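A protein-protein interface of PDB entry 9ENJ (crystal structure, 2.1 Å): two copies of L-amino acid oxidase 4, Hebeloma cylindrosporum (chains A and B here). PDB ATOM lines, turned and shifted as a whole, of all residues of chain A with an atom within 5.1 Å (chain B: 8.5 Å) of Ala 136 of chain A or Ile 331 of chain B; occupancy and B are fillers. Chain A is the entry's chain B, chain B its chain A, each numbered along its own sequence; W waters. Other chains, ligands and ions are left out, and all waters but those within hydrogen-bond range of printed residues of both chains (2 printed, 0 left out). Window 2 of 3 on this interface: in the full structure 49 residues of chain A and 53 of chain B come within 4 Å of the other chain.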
ATOM      1  N   ASN A 120       7.786  23.363  -8.696  1.00  0.00           N
ATOM      2  CA  ASN A 120       7.200  23.013  -7.401  1.00  0.00           C
ATOM      3  C   ASN A 120       7.984  23.618  -6.242  1.00  0.00           C
ATOM      4  O   ASN A 120       8.085  23.022  -5.165  1.00  0.00           O
ATOM      5  CB  ASN A 120       7.097  21.493  -7.241  1.00  0.00           C
ATOM      6  CG  ASN A 120       6.275  20.847  -8.339  1.00  0.00           C
ATOM      7  OD1 ASN A 120       5.162  21.282  -8.637  1.00  0.00           O
ATOM      8  ND2 ASN A 120       6.827  19.815  -8.961  1.00  0.00           N
ATOM      9  N   PHE A 132      12.404  17.431  -7.939  1.00  0.00           N
ATOM     10  CA  PHE A 132      11.462  18.547  -7.867  1.00  0.00           C
ATOM     11  C   PHE A 132      10.196  18.158  -7.106  1.00  0.00           C
ATOM     12  O   PHE A 132       9.078  18.517  -7.484  1.00  0.00           O
ATOM     13  CB  PHE A 132      11.123  19.063  -9.265  1.00  0.00           C
ATOM     14  CG  PHE A 132      12.329  19.453 -10.069  1.00  0.00           C
ATOM     15  CD1 PHE A 132      12.910  20.700  -9.908  1.00  0.00           C
ATOM     16  CD2 PHE A 132      12.887  18.572 -10.979  1.00  0.00           C
ATOM     17  CE1 PHE A 132      14.022  21.060 -10.642  1.00  0.00           C
ATOM     18  CE2 PHE A 132      13.999  18.928 -11.716  1.00  0.00           C
ATOM     19  CZ  PHE A 132      14.567  20.174 -11.546  1.00  0.00           C
ATOM     20  N   ASP A 133      10.378  17.427  -6.007  1.00  0.00           N
ATOM     21  CA  ASP A 133       9.290  17.036  -5.115  1.00  0.00           C
ATOM     22  C   ASP A 133       8.245  16.162  -5.806  1.00  0.00           C
ATOM     23  O   ASP A 133       7.101  16.078  -5.344  1.00  0.00           O
ATOM     24  CB  ASP A 133       8.617  18.280  -4.518  1.00  0.00           C
ATOM     25  CG  ASP A 133       8.100  18.056  -3.108  1.00  0.00           C
ATOM     26  OD1 ASP A 133       8.592  17.133  -2.420  1.00  0.00           O
ATOM     27  OD2 ASP A 133       7.197  18.809  -2.686  1.00  0.00           O
ATOM     28  N   ALA A 134       8.615  15.496  -6.900  1.00  0.00           N
ATOM     29  CA  ALA A 134       7.664  14.628  -7.590  1.00  0.00           C
ATOM     30  C   ALA A 134       7.075  13.542  -6.696  1.00  0.00           C
ATOM     31  O   ALA A 134       5.890  13.209  -6.879  1.00  0.00           O
ATOM     32  CB  ALA A 134       8.334  13.998  -8.819  1.00  0.00           C
ATOM     33  N   PRO A 135       7.808  12.947  -5.752  1.00  0.00           N
ATOM     34  CA  PRO A 135       7.173  11.955  -4.868  1.00  0.00           C
ATOM     35  C   PRO A 135       5.942  12.488  -4.159  1.00  0.00           C
ATOM     36  O   PRO A 135       4.979  11.737  -3.956  1.00  0.00           O
ATOM     37  CB  PRO A 135       8.293  11.600  -3.879  1.00  0.00           C
ATOM     38  CG  PRO A 135       9.549  11.848  -4.634  1.00  0.00           C
ATOM     39  CD  PRO A 135       9.264  13.033  -5.526  1.00  0.00           C
ATOM     40  N   ALA A 136       5.930  13.770  -3.789  1.00  0.00           N
ATOM     41  CA  ALA A 136       4.744  14.350  -3.171  1.00  0.00           C
ATOM     42  C   ALA A 136       3.578  14.441  -4.145  1.00  0.00           C
ATOM     43  O   ALA A 136       2.428  14.539  -3.704  1.00  0.00           O
ATOM     44  CB  ALA A 136       5.064  15.736  -2.611  1.00  0.00           C
ATOM     45  N   LEU A 137       3.845  14.407  -5.453  1.00  0.00           N
ATOM     46  CA  LEU A 137       2.790  14.359  -6.456  1.00  0.00           C
ATOM     47  C   LEU A 137       2.274  12.948  -6.710  1.00  0.00           C
ATOM     48  O   LEU A 137       1.311  12.787  -7.467  1.00  0.00           O
ATOM     49  CB  LEU A 137       3.288  14.943  -7.780  1.00  0.00           C
ATOM     50  CG  LEU A 137       3.156  16.451  -7.975  1.00  0.00           C
ATOM     51  CD1 LEU A 137       3.971  16.892  -9.180  1.00  0.00           C
ATOM     52  CD2 LEU A 137       1.698  16.853  -8.138  1.00  0.00           C
ATOM     53  N   GLY A 138       2.892  11.930  -6.120  1.00  0.00           N
ATOM     54  CA  GLY A 138       2.511  10.561  -6.385  1.00  0.00           C
ATOM     55  C   GLY A 138       3.268   9.892  -7.507  1.00  0.00           C
ATOM     56  O   GLY A 138       2.860   8.810  -7.945  1.00  0.00           O
ATOM     57  N   LYS B 328       0.575  28.217   1.532  1.00  0.00           N
ATOM     58  CA  LYS B 328       0.912  26.809   1.726  1.00  0.00           C
ATOM     59  C   LYS B 328      -0.020  25.889   0.940  1.00  0.00           C
ATOM     60  O   LYS B 328      -0.599  24.941   1.475  1.00  0.00           O
ATOM     61  CB  LYS B 328       0.916  26.452   3.213  1.00  0.00           C
ATOM     62  CG  LYS B 328       1.978  27.201   4.000  1.00  0.00           C
ATOM     63  CD  LYS B 328       2.131  26.664   5.413  1.00  0.00           C
ATOM     64  CE  LYS B 328       0.890  26.899   6.249  1.00  0.00           C
ATOM     65  NZ  LYS B 328       1.129  26.536   7.674  1.00  0.00           N
ATOM     66  N   LEU B 329      -0.161  26.180  -0.350  1.00  0.00           N
ATOM     67  CA  LEU B 329      -0.813  25.237  -1.247  1.00  0.00           C
ATOM     68  C   LEU B 329       0.010  23.957  -1.317  1.00  0.00           C
ATOM     69  O   LEU B 329       1.244  23.994  -1.309  1.00  0.00           O
ATOM     70  CB  LEU B 329      -0.962  25.838  -2.646  1.00  0.00           C
ATOM     71  CG  LEU B 329      -2.148  26.770  -2.902  1.00  0.00           C
ATOM     72  CD1 LEU B 329      -2.061  28.027  -2.058  1.00  0.00           C
ATOM     73  CD2 LEU B 329      -2.223  27.119  -4.386  1.00  0.00           C
ATOM     74  N   ASP B 330      -0.671  22.816  -1.348  1.00  0.00           N
ATOM     75  CA  ASP B 330       0.060  21.578  -1.562  1.00  0.00           C
ATOM     76  C   ASP B 330       0.432  21.454  -3.040  1.00  0.00           C
ATOM     77  O   ASP B 330      -0.051  22.197  -3.899  1.00  0.00           O
ATOM     78  CB  ASP B 330      -0.743  20.369  -1.078  1.00  0.00           C
ATOM     79  CG  ASP B 330      -2.002  20.131  -1.879  1.00  0.00           C
ATOM     80  OD1 ASP B 330      -1.908  19.942  -3.110  1.00  0.00           O
ATOM     81  OD2 ASP B 330      -3.092  20.104  -1.268  1.00  0.00           O
ATOM     82  N   ILE B 331       1.312  20.496  -3.331  1.00  0.00           N
ATOM     83  CA  ILE B 331       1.908  20.414  -4.659  1.00  0.00           C
ATOM     84  C   ILE B 331       0.854  20.156  -5.727  1.00  0.00           C
ATOM     85  O   ILE B 331       1.025  20.554  -6.886  1.00  0.00           O
ATOM     86  CB  ILE B 331       3.014  19.338  -4.670  1.00  0.00           C
ATOM     87  CG1 ILE B 331       3.812  19.415  -5.972  1.00  0.00           C
ATOM     88  CG2 ILE B 331       2.416  17.947  -4.472  1.00  0.00           C
ATOM     89  CD1 ILE B 331       5.119  18.654  -5.924  1.00  0.00           C
ATOM     90  N   VAL B 332      -0.247  19.492  -5.369  1.00  0.00           N
ATOM     91  CA  VAL B 332      -1.296  19.249  -6.357  1.00  0.00           C
ATOM     92  C   VAL B 332      -2.075  20.529  -6.627  1.00  0.00           C
ATOM     93  O   VAL B 332      -2.390  20.849  -7.778  1.00  0.00           O
ATOM     94  CB  VAL B 332      -2.226  18.113  -5.893  1.00  0.00           C
ATOM     95  CG1 VAL B 332      -3.216  17.763  -6.993  1.00  0.00           C
ATOM     96  CG2 VAL B 332      -1.423  16.887  -5.489  1.00  0.00           C
ATOM     97  N   GLN B 333      -2.388  21.289  -5.573  1.00  0.00           N
ATOM     98  CA  GLN B 333      -3.128  22.533  -5.753  1.00  0.00           C
ATOM     99  C   GLN B 333      -2.368  23.511  -6.642  1.00  0.00           C
ATOM    100  O   GLN B 333      -2.956  24.132  -7.535  1.00  0.00           O
ATOM    101  CB  GLN B 333      -3.419  23.169  -4.390  1.00  0.00           C
ATOM    102  CG  GLN B 333      -4.355  22.354  -3.509  1.00  0.00           C
ATOM    103  CD  GLN B 333      -4.509  22.939  -2.116  1.00  0.00           C
ATOM    104  OE1 GLN B 333      -3.530  23.339  -1.484  1.00  0.00           O
ATOM    105  NE2 GLN B 333      -5.746  22.998  -1.633  1.00  0.00           N
ATOM    106  N   SER B 334      -1.061  23.669  -6.412  1.00  0.00           N
ATOM    107  CA  SER B 334      -0.295  24.637  -7.193  1.00  0.00           C
ATOM    108  C   SER B 334      -0.210  24.223  -8.658  1.00  0.00           C
ATOM    109  O   SER B 334      -0.254  25.075  -9.553  1.00  0.00           O
ATOM    110  CB  SER B 334       1.103  24.809  -6.598  1.00  0.00           C
ATOM    111  OG  SER B 334       1.800  23.577  -6.550  1.00  0.00           O
ATOM    112  N   ASN B 335      -0.079  22.922  -8.925  1.00  0.00           N
ATOM    113  CA  ASN B 335      -0.122  22.456 -10.306  1.00  0.00           C
ATOM    114  C   ASN B 335      -1.511  22.612 -10.904  1.00  0.00           C
ATOM    115  O   ASN B 335      -1.641  22.903 -12.098  1.00  0.00           O
ATOM    116  CB  ASN B 335       0.332  21.000 -10.384  1.00  0.00           C
ATOM    117  CG  ASN B 335       1.840  20.865 -10.414  1.00  0.00           C
ATOM    118  OD1 ASN B 335       2.465  21.028 -11.462  1.00  0.00           O
ATOM    119  ND2 ASN B 335       2.438  20.591  -9.260  1.00  0.00           N
ATOM    120  N   ALA B 336      -2.557  22.443 -10.094  1.00  0.00           N
ATOM    121  CA  ALA B 336      -3.917  22.588 -10.604  1.00  0.00           C
ATOM    122  C   ALA B 336      -4.175  24.008 -11.093  1.00  0.00           C
ATOM    123  O   ALA B 336      -4.881  24.213 -12.088  1.00  0.00           O
ATOM    124  CB  ALA B 336      -4.922  22.201  -9.520  1.00  0.00           C
ATOM    125  N   LEU B 337      -3.624  25.006 -10.395  1.00  0.00           N
ATOM    126  CA  LEU B 337      -3.796  26.388 -10.835  1.00  0.00           C
ATOM    127  C   LEU B 337      -3.281  26.580 -12.255  1.00  0.00           C
ATOM    128  O   LEU B 337      -3.854  27.351 -13.033  1.00  0.00           O
ATOM    129  CB  LEU B 337      -3.071  27.342  -9.885  1.00  0.00           C
ATOM    130  CG  LEU B 337      -3.565  27.437  -8.445  1.00  0.00           C
ATOM    131  CD1 LEU B 337      -2.709  28.433  -7.674  1.00  0.00           C
ATOM    132  CD2 LEU B 337      -5.036  27.836  -8.393  1.00  0.00           C
ATOM    133  N   ARG B 338      -2.207  25.875 -12.614  1.00  0.00           N
ATOM    134  CA  ARG B 338      -1.606  26.048 -13.932  1.00  0.00           C
ATOM    135  C   ARG B 338      -2.308  25.204 -14.989  1.00  0.00           C
ATOM    136  O   ARG B 338      -2.580  25.691 -16.093  1.00  0.00           O
ATOM    137  CB  ARG B 338      -0.115  25.696 -13.872  1.00  0.00           C
ATOM    138  CG  ARG B 338       0.603  25.720 -15.222  1.00  0.00           C
ATOM    139  CD  ARG B 338       2.084  25.388 -15.087  1.00  0.00           C
ATOM    140  NE  ARG B 338       2.318  24.077 -14.487  1.00  0.00           N
ATOM    141  CZ  ARG B 338       2.306  22.929 -15.151  1.00  0.00           C
ATOM    142  NH1 ARG B 338       2.057  22.882 -16.450  1.00  0.00           N
ATOM    143  NH2 ARG B 338       2.552  21.797 -14.495  1.00  0.00           N
ATOM    144  N   LEU B 480      -6.952  16.739 -10.977  1.00  0.00           N
ATOM    145  CA  LEU B 480      -6.580  17.987 -10.325  1.00  0.00           C
ATOM    146  C   LEU B 480      -7.748  18.751  -9.726  1.00  0.00           C
ATOM    147  O   LEU B 480      -7.527  19.576  -8.833  1.00  0.00           O
ATOM    148  CB  LEU B 480      -5.863  18.912 -11.322  1.00  0.00           C
ATOM    149  CG  LEU B 480      -4.550  18.383 -11.901  1.00  0.00           C
ATOM    150  CD1 LEU B 480      -4.137  19.201 -13.104  1.00  0.00           C
ATOM    151  CD2 LEU B 480      -3.452  18.396 -10.858  1.00  0.00           C
ATOM    152  N   SER B 483      -8.213  18.767  -5.785  1.00  0.00           N
ATOM    153  CA  SER B 483      -7.221  19.422  -4.936  1.00  0.00           C
ATOM    154  C   SER B 483      -7.676  20.819  -4.528  1.00  0.00           C
ATOM    155  O   SER B 483      -7.469  21.238  -3.384  1.00  0.00           O
ATOM    156  CB  SER B 483      -5.873  19.494  -5.654  1.00  0.00           C
ATOM    157  OG  SER B 483      -5.890  20.453  -6.698  1.00  0.00           O
ATOM    158  N   ARG B 486     -10.212  21.251  -1.636  1.00  0.00           N
ATOM    159  CA  ARG B 486      -9.658  21.352  -0.297  1.00  0.00           C
ATOM    160  C   ARG B 486      -9.203  22.788  -0.039  1.00  0.00           C
ATOM    161  O   ARG B 486      -8.772  23.485  -0.964  1.00  0.00           O
ATOM    162  CB  ARG B 486      -8.470  20.412  -0.129  1.00  0.00           C
ATOM    163  CG  ARG B 486      -8.774  18.945  -0.350  1.00  0.00           C
ATOM    164  CD  ARG B 486      -7.582  18.080   0.040  1.00  0.00           C
ATOM    165  NE  ARG B 486      -6.391  18.392  -0.744  1.00  0.00           N
ATOM    166  CZ  ARG B 486      -6.064  17.798  -1.885  1.00  0.00           C
ATOM    167  NH1 ARG B 486      -6.828  16.860  -2.423  1.00  0.00           N
ATOM    168  NH2 ARG B 486      -4.945  18.159  -2.508  1.00  0.00           N
HETATM  169  O   HOH W   1       5.131  21.433 -11.901  1.00  0.00           O
HETATM  170  O   HOH W   2       3.916  23.368  -8.367  1.00  0.00           O
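The side-chain amide oxygen of Asn 120 of chain A sits at hydrogen-bond distance from the side-chain amide nitrogen of Asn 335 of chain B, at 2.9 Å.
The side-chain amide nitrogen (ND2) of Asn 120 of chain A is in hydrogen-bond range of the backbone carbonyl oxygen (O) of Phe 132 of chain A (3.0 Å). ND2 of Asn 335 of chain B lies within hydrogen-bond range of O of Ile 331 of chain B, at 2.8 Å. The guanidinium group (NH2) of Arg 338 of chain B sits at hydrogen-bond distance from the side-chain amide oxygen (OD1) of Asn 335 of chain B. The backbone carbonyl oxygen of Ile 331 of chain B lies within hydrogen-bond range of the side-chain hydroxyl of Ser 334 of chain B (3.1 Å).
Among the printed residues, pairs that only touch across the chains: Asp 133 of chain A with Ile 331 of chain B, Asn 120 of chain A with Ile 331 of chain B, Ala 136 of chain A with Ile 331 of chain B, Leu 137 of chain A with Ile 331 of chain B and Leu 137 of chain A with Asn 335 of chain B.
Of the printed residues of chain B, Asn 120 of chain A touches Ile 331 (3.5 Å) and Asn 335 (2.9 Å). Of the printed residues of chain B, Asp 133 of chain A touches Ile 331 (3.3 Å). No residue of chain B comes within 4 Å of Pro 135 of chain A. Of the printed residues of chain B, Ala 136 of chain A touches Ile 331 (3.5 Å). Of chain B, only Ile 331 and Asn 335 come within 4 Å of Leu 137 of chain A. Of the printed residues of chain A, Asn 335 of chain B touches Asn 120 and Leu 137. The nearest residue of chain B that does not touch Ala 136 of chain A is Val 332 of chain B (4.9 Å). The nearest printed residue of chain B that does not touch Asp 133 of chain A is Asp 330 of chain B (7.3 Å).
Printed residues of chain B that touch a printed residue of chain A: Ile 331 and Asn 335. Hydrophobic or aromatic side chains of chain B within 4 Å of the printed part of chain A: Ile 331.
No position is printed for both chains.
Water W2 lies within hydrogen-bond range of OD1 of Asn 120 of chain A (2.4 Å), OG of Ser 334 of chain B (2.8 Å) and ND2 of Asn 335 of chain B (3.3 Å). Water W1 lies within hydrogen-bond range of the side-chain amide oxygen (OD1) of Asn 335 of chain B (2.7 Å) and the side-chain amide oxygen (OD1) of Asn 120 of chain A (3.3 Å).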
